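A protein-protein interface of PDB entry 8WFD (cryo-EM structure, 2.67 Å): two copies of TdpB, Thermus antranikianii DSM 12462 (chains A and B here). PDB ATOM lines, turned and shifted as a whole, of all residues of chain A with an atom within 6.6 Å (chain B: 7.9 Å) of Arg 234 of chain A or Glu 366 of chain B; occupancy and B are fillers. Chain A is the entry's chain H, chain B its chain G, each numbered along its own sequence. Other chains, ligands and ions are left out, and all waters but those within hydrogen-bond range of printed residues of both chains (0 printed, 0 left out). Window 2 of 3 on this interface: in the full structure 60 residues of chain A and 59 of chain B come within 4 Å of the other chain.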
ATOM      1  N   ASP A  33     -25.998   5.985  15.268  1.00  0.00           N
ATOM      2  CA  ASP A  33     -26.832   5.467  14.191  1.00  0.00           C
ATOM      3  C   ASP A  33     -27.336   6.591  13.295  1.00  0.00           C
ATOM      4  O   ASP A  33     -27.465   6.413  12.081  1.00  0.00           O
ATOM      5  CB  ASP A  33     -28.002   4.674  14.769  1.00  0.00           C
ATOM      6  CG  ASP A  33     -28.679   3.804  13.734  1.00  0.00           C
ATOM      7  OD1 ASP A  33     -28.033   3.488  12.713  1.00  0.00           O
ATOM      8  OD2 ASP A  33     -29.857   3.439  13.937  1.00  0.00           O
ATOM      9  N   TYR A  36     -24.516   7.322  11.005  1.00  0.00           N
ATOM     10  CA  TYR A  36     -24.387   6.269  10.002  1.00  0.00           C
ATOM     11  C   TYR A  36     -25.469   6.390   8.934  1.00  0.00           C
ATOM     12  O   TYR A  36     -25.212   6.166   7.746  1.00  0.00           O
ATOM     13  CB  TYR A  36     -24.436   4.892  10.657  1.00  0.00           C
ATOM     14  CG  TYR A  36     -24.253   3.765   9.667  1.00  0.00           C
ATOM     15  CD1 TYR A  36     -23.178   3.760   8.789  1.00  0.00           C
ATOM     16  CD2 TYR A  36     -25.157   2.717   9.599  1.00  0.00           C
ATOM     17  CE1 TYR A  36     -23.006   2.737   7.877  1.00  0.00           C
ATOM     18  CE2 TYR A  36     -24.993   1.691   8.691  1.00  0.00           C
ATOM     19  CZ  TYR A  36     -23.917   1.706   7.832  1.00  0.00           C
ATOM     20  OH  TYR A  36     -23.751   0.683   6.925  1.00  0.00           O
ATOM     21  N   LEU A  39     -24.476   8.995   6.578  1.00  0.00           N
ATOM     22  CA  LEU A  39     -23.469   8.473   5.658  1.00  0.00           C
ATOM     23  C   LEU A  39     -24.099   7.621   4.562  1.00  0.00           C
ATOM     24  O   LEU A  39     -23.687   7.692   3.399  1.00  0.00           O
ATOM     25  CB  LEU A  39     -22.422   7.665   6.420  1.00  0.00           C
ATOM     26  CG  LEU A  39     -21.408   8.500   7.193  1.00  0.00           C
ATOM     27  CD1 LEU A  39     -20.483   7.612   8.008  1.00  0.00           C
ATOM     28  CD2 LEU A  39     -20.625   9.349   6.210  1.00  0.00           C
ATOM     29  N   LEU A 230     -14.226   8.354  11.539  1.00  0.00           N
ATOM     30  CA  LEU A 230     -13.861   7.003  11.144  1.00  0.00           C
ATOM     31  C   LEU A 230     -15.026   6.031  11.248  1.00  0.00           C
ATOM     32  O   LEU A 230     -14.808   4.814  11.245  1.00  0.00           O
ATOM     33  CB  LEU A 230     -12.681   6.505  11.982  1.00  0.00           C
ATOM     34  CG  LEU A 230     -11.290   6.908  11.489  1.00  0.00           C
ATOM     35  CD1 LEU A 230     -10.983   6.245  10.156  1.00  0.00           C
ATOM     36  CD2 LEU A 230     -11.174   8.418  11.375  1.00  0.00           C
ATOM     37  N   VAL A 231     -16.256   6.543  11.344  1.00  0.00           N
ATOM     38  CA  VAL A 231     -17.435   5.717  11.136  1.00  0.00           C
ATOM     39  C   VAL A 231     -17.416   5.057   9.767  1.00  0.00           C
ATOM     40  O   VAL A 231     -18.179   4.119   9.521  1.00  0.00           O
ATOM     41  CB  VAL A 231     -18.717   6.562  11.324  1.00  0.00           C
ATOM     42  CG1 VAL A 231     -19.945   5.788  10.876  1.00  0.00           C
ATOM     43  CG2 VAL A 231     -18.858   6.992  12.774  1.00  0.00           C
ATOM     44  N   MET A 232     -16.539   5.520   8.871  1.00  0.00           N
ATOM     45  CA  MET A 232     -16.326   4.840   7.601  1.00  0.00           C
ATOM     46  C   MET A 232     -15.859   3.407   7.798  1.00  0.00           C
ATOM     47  O   MET A 232     -16.003   2.590   6.881  1.00  0.00           O
ATOM     48  CB  MET A 232     -15.304   5.604   6.757  1.00  0.00           C
ATOM     49  CG  MET A 232     -15.518   7.106   6.715  1.00  0.00           C
ATOM     50  SD  MET A 232     -16.711   7.622   5.468  1.00  0.00           S
ATOM     51  CE  MET A 232     -17.556   8.928   6.351  1.00  0.00           C
ATOM     52  N   ALA A 233     -15.301   3.081   8.968  1.00  0.00           N
ATOM     53  CA  ALA A 233     -15.000   1.688   9.275  1.00  0.00           C
ATOM     54  C   ALA A 233     -16.228   0.822   9.033  1.00  0.00           C
ATOM     55  O   ALA A 233     -16.132  -0.281   8.486  1.00  0.00           O
ATOM     56  CB  ALA A 233     -14.517   1.558  10.719  1.00  0.00           C
ATOM     57  N   ARG A 234     -17.392   1.316   9.438  1.00  0.00           N
ATOM     58  CA  ARG A 234     -18.648   0.788   8.939  1.00  0.00           C
ATOM     59  C   ARG A 234     -18.990   1.465   7.617  1.00  0.00           C
ATOM     60  O   ARG A 234     -18.578   2.598   7.351  1.00  0.00           O
ATOM     61  CB  ARG A 234     -19.772   1.008   9.950  1.00  0.00           C
ATOM     62  CG  ARG A 234     -21.115   0.462   9.500  1.00  0.00           C
ATOM     63  CD  ARG A 234     -22.197   0.739  10.527  1.00  0.00           C
ATOM     64  NE  ARG A 234     -22.094  -0.143  11.682  1.00  0.00           N
ATOM     65  CZ  ARG A 234     -23.117  -0.492  12.450  1.00  0.00           C
ATOM     66  NH1 ARG A 234     -24.341  -0.052  12.210  1.00  0.00           N
ATOM     67  NH2 ARG A 234     -22.906  -1.300  13.484  1.00  0.00           N
ATOM     68  N   LEU A 235     -19.752   0.763   6.786  1.00  0.00           N
ATOM     69  CA  LEU A 235     -20.150   1.165   5.444  1.00  0.00           C
ATOM     70  C   LEU A 235     -19.020   0.981   4.429  1.00  0.00           C
ATOM     71  O   LEU A 235     -19.258   1.156   3.235  1.00  0.00           O
ATOM     72  CB  LEU A 235     -20.654   2.620   5.378  1.00  0.00           C
ATOM     73  CG  LEU A 235     -21.334   3.108   4.099  1.00  0.00           C
ATOM     74  CD1 LEU A 235     -22.440   4.085   4.442  1.00  0.00           C
ATOM     75  CD2 LEU A 235     -20.325   3.765   3.175  1.00  0.00           C
ATOM     76  N   PHE A 236     -17.806   0.624   4.852  1.00  0.00           N
ATOM     77  CA  PHE A 236     -16.812   0.098   3.925  1.00  0.00           C
ATOM     78  C   PHE A 236     -16.930  -1.407   3.757  1.00  0.00           C
ATOM     79  O   PHE A 236     -16.503  -1.944   2.727  1.00  0.00           O
ATOM     80  CB  PHE A 236     -15.396   0.471   4.370  1.00  0.00           C
ATOM     81  CG  PHE A 236     -15.064   1.920   4.166  1.00  0.00           C
ATOM     82  CD1 PHE A 236     -15.844   2.705   3.334  1.00  0.00           C
ATOM     83  CD2 PHE A 236     -13.970   2.495   4.788  1.00  0.00           C
ATOM     84  CE1 PHE A 236     -15.544   4.035   3.131  1.00  0.00           C
ATOM     85  CE2 PHE A 236     -13.666   3.828   4.590  1.00  0.00           C
ATOM     86  CZ  PHE A 236     -14.455   4.599   3.760  1.00  0.00           C
ATOM     87  N   ALA A 237     -17.485  -2.100   4.745  1.00  0.00           N
ATOM     88  CA  ALA A 237     -17.990  -3.440   4.500  1.00  0.00           C
ATOM     89  C   ALA A 237     -19.139  -3.353   3.505  1.00  0.00           C
ATOM     90  O   ALA A 237     -19.918  -2.397   3.518  1.00  0.00           O
ATOM     91  CB  ALA A 237     -18.452  -4.087   5.806  1.00  0.00           C
ATOM     92  N   GLU A 238     -19.238  -4.354   2.630  1.00  0.00           N
ATOM     93  CA  GLU A 238     -20.155  -4.312   1.491  1.00  0.00           C
ATOM     94  C   GLU A 238     -20.103  -2.945   0.807  1.00  0.00           C
ATOM     95  O   GLU A 238     -21.115  -2.264   0.632  1.00  0.00           O
ATOM     96  CB  GLU A 238     -21.589  -4.673   1.903  1.00  0.00           C
ATOM     97  CG  GLU A 238     -22.310  -3.649   2.778  1.00  0.00           C
ATOM     98  CD  GLU A 238     -22.132  -3.901   4.265  1.00  0.00           C
ATOM     99  OE1 GLU A 238     -21.255  -4.708   4.639  1.00  0.00           O
ATOM    100  OE2 GLU A 238     -22.869  -3.281   5.061  1.00  0.00           O
ATOM    101  N   PRO A 287     -10.693  -3.715  10.412  1.00  0.00           N
ATOM    102  CA  PRO A 287     -11.767  -2.816   9.952  1.00  0.00           C
ATOM    103  C   PRO A 287     -11.277  -1.503   9.365  1.00  0.00           C
ATOM    104  O   PRO A 287     -11.885  -0.998   8.415  1.00  0.00           O
ATOM    105  CB  PRO A 287     -12.598  -2.586  11.224  1.00  0.00           C
ATOM    106  CG  PRO A 287     -12.176  -3.650  12.183  1.00  0.00           C
ATOM    107  CD  PRO A 287     -10.760  -3.971  11.859  1.00  0.00           C
ATOM    108  N   GLN A 288     -10.197  -0.932   9.896  1.00  0.00           N
ATOM    109  CA  GLN A 288      -9.843   0.443   9.564  1.00  0.00           C
ATOM    110  C   GLN A 288      -8.474   0.559   8.909  1.00  0.00           C
ATOM    111  O   GLN A 288      -7.671   1.416   9.291  1.00  0.00           O
ATOM    112  CB  GLN A 288      -9.892   1.316  10.819  1.00  0.00           C
ATOM    113  CG  GLN A 288     -11.256   1.369  11.480  1.00  0.00           C
ATOM    114  CD  GLN A 288     -11.342   2.433  12.553  1.00  0.00           C
ATOM    115  OE1 GLN A 288     -10.428   3.241  12.717  1.00  0.00           O
ATOM    116  NE2 GLN A 288     -12.443   2.439  13.290  1.00  0.00           N
ATOM    117  N   LEU B 349     -20.978  -4.069  30.064  1.00  0.00           N
ATOM    118  CA  LEU B 349     -21.744  -4.481  28.894  1.00  0.00           C
ATOM    119  C   LEU B 349     -22.778  -5.536  29.263  1.00  0.00           C
ATOM    120  O   LEU B 349     -23.914  -5.501  28.777  1.00  0.00           O
ATOM    121  CB  LEU B 349     -20.804  -4.997  27.805  1.00  0.00           C
ATOM    122  CG  LEU B 349     -21.416  -5.151  26.412  1.00  0.00           C
ATOM    123  CD1 LEU B 349     -20.354  -4.973  25.340  1.00  0.00           C
ATOM    124  CD2 LEU B 349     -22.103  -6.495  26.271  1.00  0.00           C
ATOM    125  N   ASP B 359     -31.048  -7.119  21.882  1.00  0.00           N
ATOM    126  CA  ASP B 359     -30.946  -6.455  20.587  1.00  0.00           C
ATOM    127  C   ASP B 359     -30.114  -5.181  20.671  1.00  0.00           C
ATOM    128  O   ASP B 359     -29.156  -5.010  19.913  1.00  0.00           O
ATOM    129  CB  ASP B 359     -32.342  -6.141  20.042  1.00  0.00           C
ATOM    130  CG  ASP B 359     -32.313  -5.672  18.598  1.00  0.00           C
ATOM    131  OD1 ASP B 359     -31.212  -5.615  18.010  1.00  0.00           O
ATOM    132  OD2 ASP B 359     -33.391  -5.360  18.052  1.00  0.00           O
ATOM    133  N   LEU B 360     -30.468  -4.279  21.589  1.00  0.00           N
ATOM    134  CA  LEU B 360     -29.730  -3.030  21.726  1.00  0.00           C
ATOM    135  C   LEU B 360     -28.300  -3.255  22.200  1.00  0.00           C
ATOM    136  O   LEU B 360     -27.460  -2.362  22.044  1.00  0.00           O
ATOM    137  CB  LEU B 360     -30.462  -2.095  22.689  1.00  0.00           C
ATOM    138  CG  LEU B 360     -29.880  -0.693  22.863  1.00  0.00           C
ATOM    139  CD1 LEU B 360     -29.817   0.022  21.525  1.00  0.00           C
ATOM    140  CD2 LEU B 360     -30.702   0.105  23.861  1.00  0.00           C
ATOM    141  N   ALA B 361     -28.003  -4.421  22.773  1.00  0.00           N
ATOM    142  CA  ALA B 361     -26.658  -4.718  23.246  1.00  0.00           C
ATOM    143  C   ALA B 361     -25.730  -5.195  22.138  1.00  0.00           C
ATOM    144  O   ALA B 361     -24.516  -4.967  22.216  1.00  0.00           O
ATOM    145  CB  ALA B 361     -26.711  -5.775  24.352  1.00  0.00           C
ATOM    146  N   LYS B 362     -26.269  -5.857  21.112  1.00  0.00           N
ATOM    147  CA  LYS B 362     -25.431  -6.371  20.034  1.00  0.00           C
ATOM    148  C   LYS B 362     -24.772  -5.240  19.252  1.00  0.00           C
ATOM    149  O   LYS B 362     -23.594  -5.330  18.882  1.00  0.00           O
ATOM    150  CB  LYS B 362     -26.267  -7.249  19.106  1.00  0.00           C
ATOM    151  CG  LYS B 362     -25.581  -7.626  17.806  1.00  0.00           C
ATOM    152  CD  LYS B 362     -24.583  -8.749  18.026  1.00  0.00           C
ATOM    153  CE  LYS B 362     -23.666  -8.923  16.830  1.00  0.00           C
ATOM    154  NZ  LYS B 362     -22.517  -9.809  17.153  1.00  0.00           N
ATOM    155  N   LYS B 363     -25.520  -4.167  18.987  1.00  0.00           N
ATOM    156  CA  LYS B 363     -24.978  -3.073  18.190  1.00  0.00           C
ATOM    157  C   LYS B 363     -23.902  -2.302  18.942  1.00  0.00           C
ATOM    158  O   LYS B 363     -22.971  -1.782  18.319  1.00  0.00           O
ATOM    159  CB  LYS B 363     -26.103  -2.140  17.746  1.00  0.00           C
ATOM    160  CG  LYS B 363     -27.138  -2.817  16.863  1.00  0.00           C
ATOM    161  CD  LYS B 363     -28.331  -1.914  16.610  1.00  0.00           C
ATOM    162  CE  LYS B 363     -28.991  -1.502  17.913  1.00  0.00           C
ATOM    163  NZ  LYS B 363     -29.315  -2.685  18.753  1.00  0.00           N
ATOM    164  N   LEU B 364     -24.003  -2.215  20.269  1.00  0.00           N
ATOM    165  CA  LEU B 364     -22.923  -1.605  21.040  1.00  0.00           C
ATOM    166  C   LEU B 364     -21.621  -2.370  20.845  1.00  0.00           C
ATOM    167  O   LEU B 364     -20.565  -1.771  20.600  1.00  0.00           O
ATOM    168  CB  LEU B 364     -23.302  -1.551  22.520  1.00  0.00           C
ATOM    169  CG  LEU B 364     -22.294  -0.905  23.474  1.00  0.00           C
ATOM    170  CD1 LEU B 364     -22.321   0.607  23.338  1.00  0.00           C
ATOM    171  CD2 LEU B 364     -22.571  -1.321  24.910  1.00  0.00           C
ATOM    172  N   THR B 365     -21.680  -3.701  20.932  1.00  0.00           N
ATOM    173  CA  THR B 365     -20.488  -4.511  20.718  1.00  0.00           C
ATOM    174  C   THR B 365     -19.981  -4.380  19.287  1.00  0.00           C
ATOM    175  O   THR B 365     -18.768  -4.344  19.056  1.00  0.00           O
ATOM    176  CB  THR B 365     -20.778  -5.975  21.052  1.00  0.00           C
ATOM    177  OG1 THR B 365     -21.477  -6.587  19.961  1.00  0.00           O
ATOM    178  CG2 THR B 365     -21.625  -6.076  22.310  1.00  0.00           C
ATOM    179  N   GLU B 366     -20.894  -4.321  18.314  1.00  0.00           N
ATOM    180  CA  GLU B 366     -20.469  -4.155  16.925  1.00  0.00           C
ATOM    181  C   GLU B 366     -19.744  -2.828  16.724  1.00  0.00           C
ATOM    182  O   GLU B 366     -18.700  -2.773  16.059  1.00  0.00           O
ATOM    183  CB  GLU B 366     -21.676  -4.259  15.994  1.00  0.00           C
ATOM    184  CG  GLU B 366     -22.294  -5.646  15.932  1.00  0.00           C
ATOM    185  CD  GLU B 366     -23.479  -5.718  14.988  1.00  0.00           C
ATOM    186  OE1 GLU B 366     -23.895  -4.659  14.471  1.00  0.00           O
ATOM    187  OE2 GLU B 366     -23.996  -6.832  14.764  1.00  0.00           O
ATOM    188  N   TRP B 367     -20.282  -1.746  17.291  1.00  0.00           N
ATOM    189  CA  TRP B 367     -19.617  -0.450  17.208  1.00  0.00           C
ATOM    190  C   TRP B 367     -18.248  -0.495  17.871  1.00  0.00           C
ATOM    191  O   TRP B 367     -17.269   0.040  17.334  1.00  0.00           O
ATOM    192  CB  TRP B 367     -20.485   0.628  17.858  1.00  0.00           C
ATOM    193  CG  TRP B 367     -21.532   1.212  16.959  1.00  0.00           C
ATOM    194  CD1 TRP B 367     -22.885   1.115  17.107  1.00  0.00           C
ATOM    195  CD2 TRP B 367     -21.313   2.001  15.784  1.00  0.00           C
ATOM    196  NE1 TRP B 367     -23.522   1.785  16.092  1.00  0.00           N
ATOM    197  CE2 TRP B 367     -22.579   2.339  15.266  1.00  0.00           C
ATOM    198  CE3 TRP B 367     -20.171   2.451  15.115  1.00  0.00           C
ATOM    199  CZ2 TRP B 367     -22.734   3.105  14.115  1.00  0.00           C
ATOM    200  CZ3 TRP B 367     -20.327   3.210  13.973  1.00  0.00           C
ATOM    201  CH2 TRP B 367     -21.599   3.530  13.484  1.00  0.00           C
ATOM    202  N   LEU B 368     -18.159  -1.129  19.042  1.00  0.00           N
ATOM    203  CA  LEU B 368     -16.873  -1.232  19.724  1.00  0.00           C
ATOM    204  C   LEU B 368     -15.865  -1.999  18.880  1.00  0.00           C
ATOM    205  O   LEU B 368     -14.695  -1.609  18.787  1.00  0.00           O
ATOM    206  CB  LEU B 368     -17.052  -1.897  21.088  1.00  0.00           C
ATOM    207  CG  LEU B 368     -17.792  -1.081  22.148  1.00  0.00           C
ATOM    208  CD1 LEU B 368     -18.143  -1.951  23.342  1.00  0.00           C
ATOM    209  CD2 LEU B 368     -16.964   0.118  22.578  1.00  0.00           C
ATOM    210  N   ARG B 369     -16.297  -3.098  18.257  1.00  0.00           N
ATOM    211  CA  ARG B 369     -15.400  -3.863  17.401  1.00  0.00           C
ATOM    212  C   ARG B 369     -14.925  -3.030  16.219  1.00  0.00           C
ATOM    213  O   ARG B 369     -13.738  -3.048  15.872  1.00  0.00           O
ATOM    214  CB  ARG B 369     -16.092  -5.130  16.904  1.00  0.00           C
ATOM    215  CG  ARG B 369     -16.644  -6.027  17.995  1.00  0.00           C
ATOM    216  CD  ARG B 369     -17.643  -7.010  17.410  1.00  0.00           C
ATOM    217  NE  ARG B 369     -18.048  -8.031  18.367  1.00  0.00           N
ATOM    218  CZ  ARG B 369     -19.108  -8.813  18.215  1.00  0.00           C
ATOM    219  NH1 ARG B 369     -19.890  -8.716  17.152  1.00  0.00           N
ATOM    220  NH2 ARG B 369     -19.391  -9.714  19.152  1.00  0.00           N
ATOM    221  N   LEU B 370     -15.839  -2.295  15.583  1.00  0.00           N
ATOM    222  CA  LEU B 370     -15.455  -1.496  14.424  1.00  0.00           C
ATOM    223  C   LEU B 370     -14.483  -0.386  14.807  1.00  0.00           C
ATOM    224  O   LEU B 370     -13.517  -0.123  14.081  1.00  0.00           O
ATOM    225  CB  LEU B 370     -16.695  -0.917  13.747  1.00  0.00           C
ATOM    226  CG  LEU B 370     -17.529  -1.918  12.950  1.00  0.00           C
ATOM    227  CD1 LEU B 370     -18.802  -1.269  12.433  1.00  0.00           C
ATOM    228  CD2 LEU B 370     -16.714  -2.496  11.809  1.00  0.00           C
ATOM    229  N   ALA B 371     -14.718   0.277  15.937  1.00  0.00           N
ATOM    230  CA  ALA B 371     -13.908   1.414  16.367  1.00  0.00           C
ATOM    231  C   ALA B 371     -13.209   1.052  17.673  1.00  0.00           C
ATOM    232  O   ALA B 371     -13.836   1.053  18.737  1.00  0.00           O
ATOM    233  CB  ALA B 371     -14.768   2.665  16.524  1.00  0.00           C
ATOM    234  N   ASP B 372     -11.913   0.760  17.588  1.00  0.00           N
ATOM    235  CA  ASP B 372     -11.109   0.388  18.753  1.00  0.00           C
ATOM    236  C   ASP B 372     -11.852  -0.559  19.689  1.00  0.00           C
ATOM    237  O   ASP B 372     -12.421  -0.133  20.693  1.00  0.00           O
ATOM    238  CB  ASP B 372     -10.664   1.638  19.521  1.00  0.00           C
ATOM    239  CG  ASP B 372      -9.496   2.348  18.858  1.00  0.00           C
ATOM    240  OD1 ASP B 372      -8.666   1.663  18.224  1.00  0.00           O
ATOM    241  OD2 ASP B 372      -9.406   3.588  18.971  1.00  0.00           O
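Among the printed residues, pairs that only touch across the chains: Arg 234 of chain A with Leu 370 of chain B (3.5 Å), Gln 288 of chain A with Ala 371 of chain B (3.6 Å), Val 231 of chain A with Trp 367 of chain B (3.8 Å), Pro 287 of chain A with Leu 370 of chain B (3.9 Å), Ala 233 of chain A with Leu 370 of chain B (3.9 Å) and Arg 234 of chain A with Trp 367 of chain B (3.98 Å).
NE2 of Gln 288 of chain A lies within hydrogen-bond range of O of Leu 370 of chain B (2.9 Å). The guanidinium group (NH2) of Arg 234 of chain A is in salt-bridge range of the side-chain carboxylate (OE1) of Glu 366 of chain B (3.6 Å).
Of the printed residues of chain B, Val 231 of chain A touches Trp 367. Of the printed residues of chain B, Arg 234 of chain A touches Glu 366, Trp 367 and Leu 370. Of the printed residues of chain B, Pro 287 of chain A touches Leu 370 (3.9 Å). Of the printed residues of chain B, Gln 288 of chain A touches Leu 370 (2.9 Å) and Ala 371 (3.6 Å). Glu 366 of chain B touches just one residue of chain A: Arg 234. Of the printed residues of chain A, Trp 367 of chain B touches Val 231 and Arg 234. Of the printed residues of chain A, Ala 371 of chain B touches Gln 288. The nearest printed residue of chain B that does not touch Arg 234 of chain A is Lys 363 of chain B (4.9 Å). The nearest printed residue of chain A that does not touch Glu 366 of chain B is Pro 287 of chain A (7.6 Å).
Hydrophobic or aromatic side chains of chain B within 4 Å of the printed part of chain A: Trp 367, Leu 370 and Ala 371. Along chain B the printed residues that touch a printed residue of chain A span positions 366 to 371. Among the printed residues, 8 pairs touch across the chains.
No position is printed for both chains. Of the 8 pairs that touch across the chains among the printed residues, none has its exchanged pair printed and touching as well.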
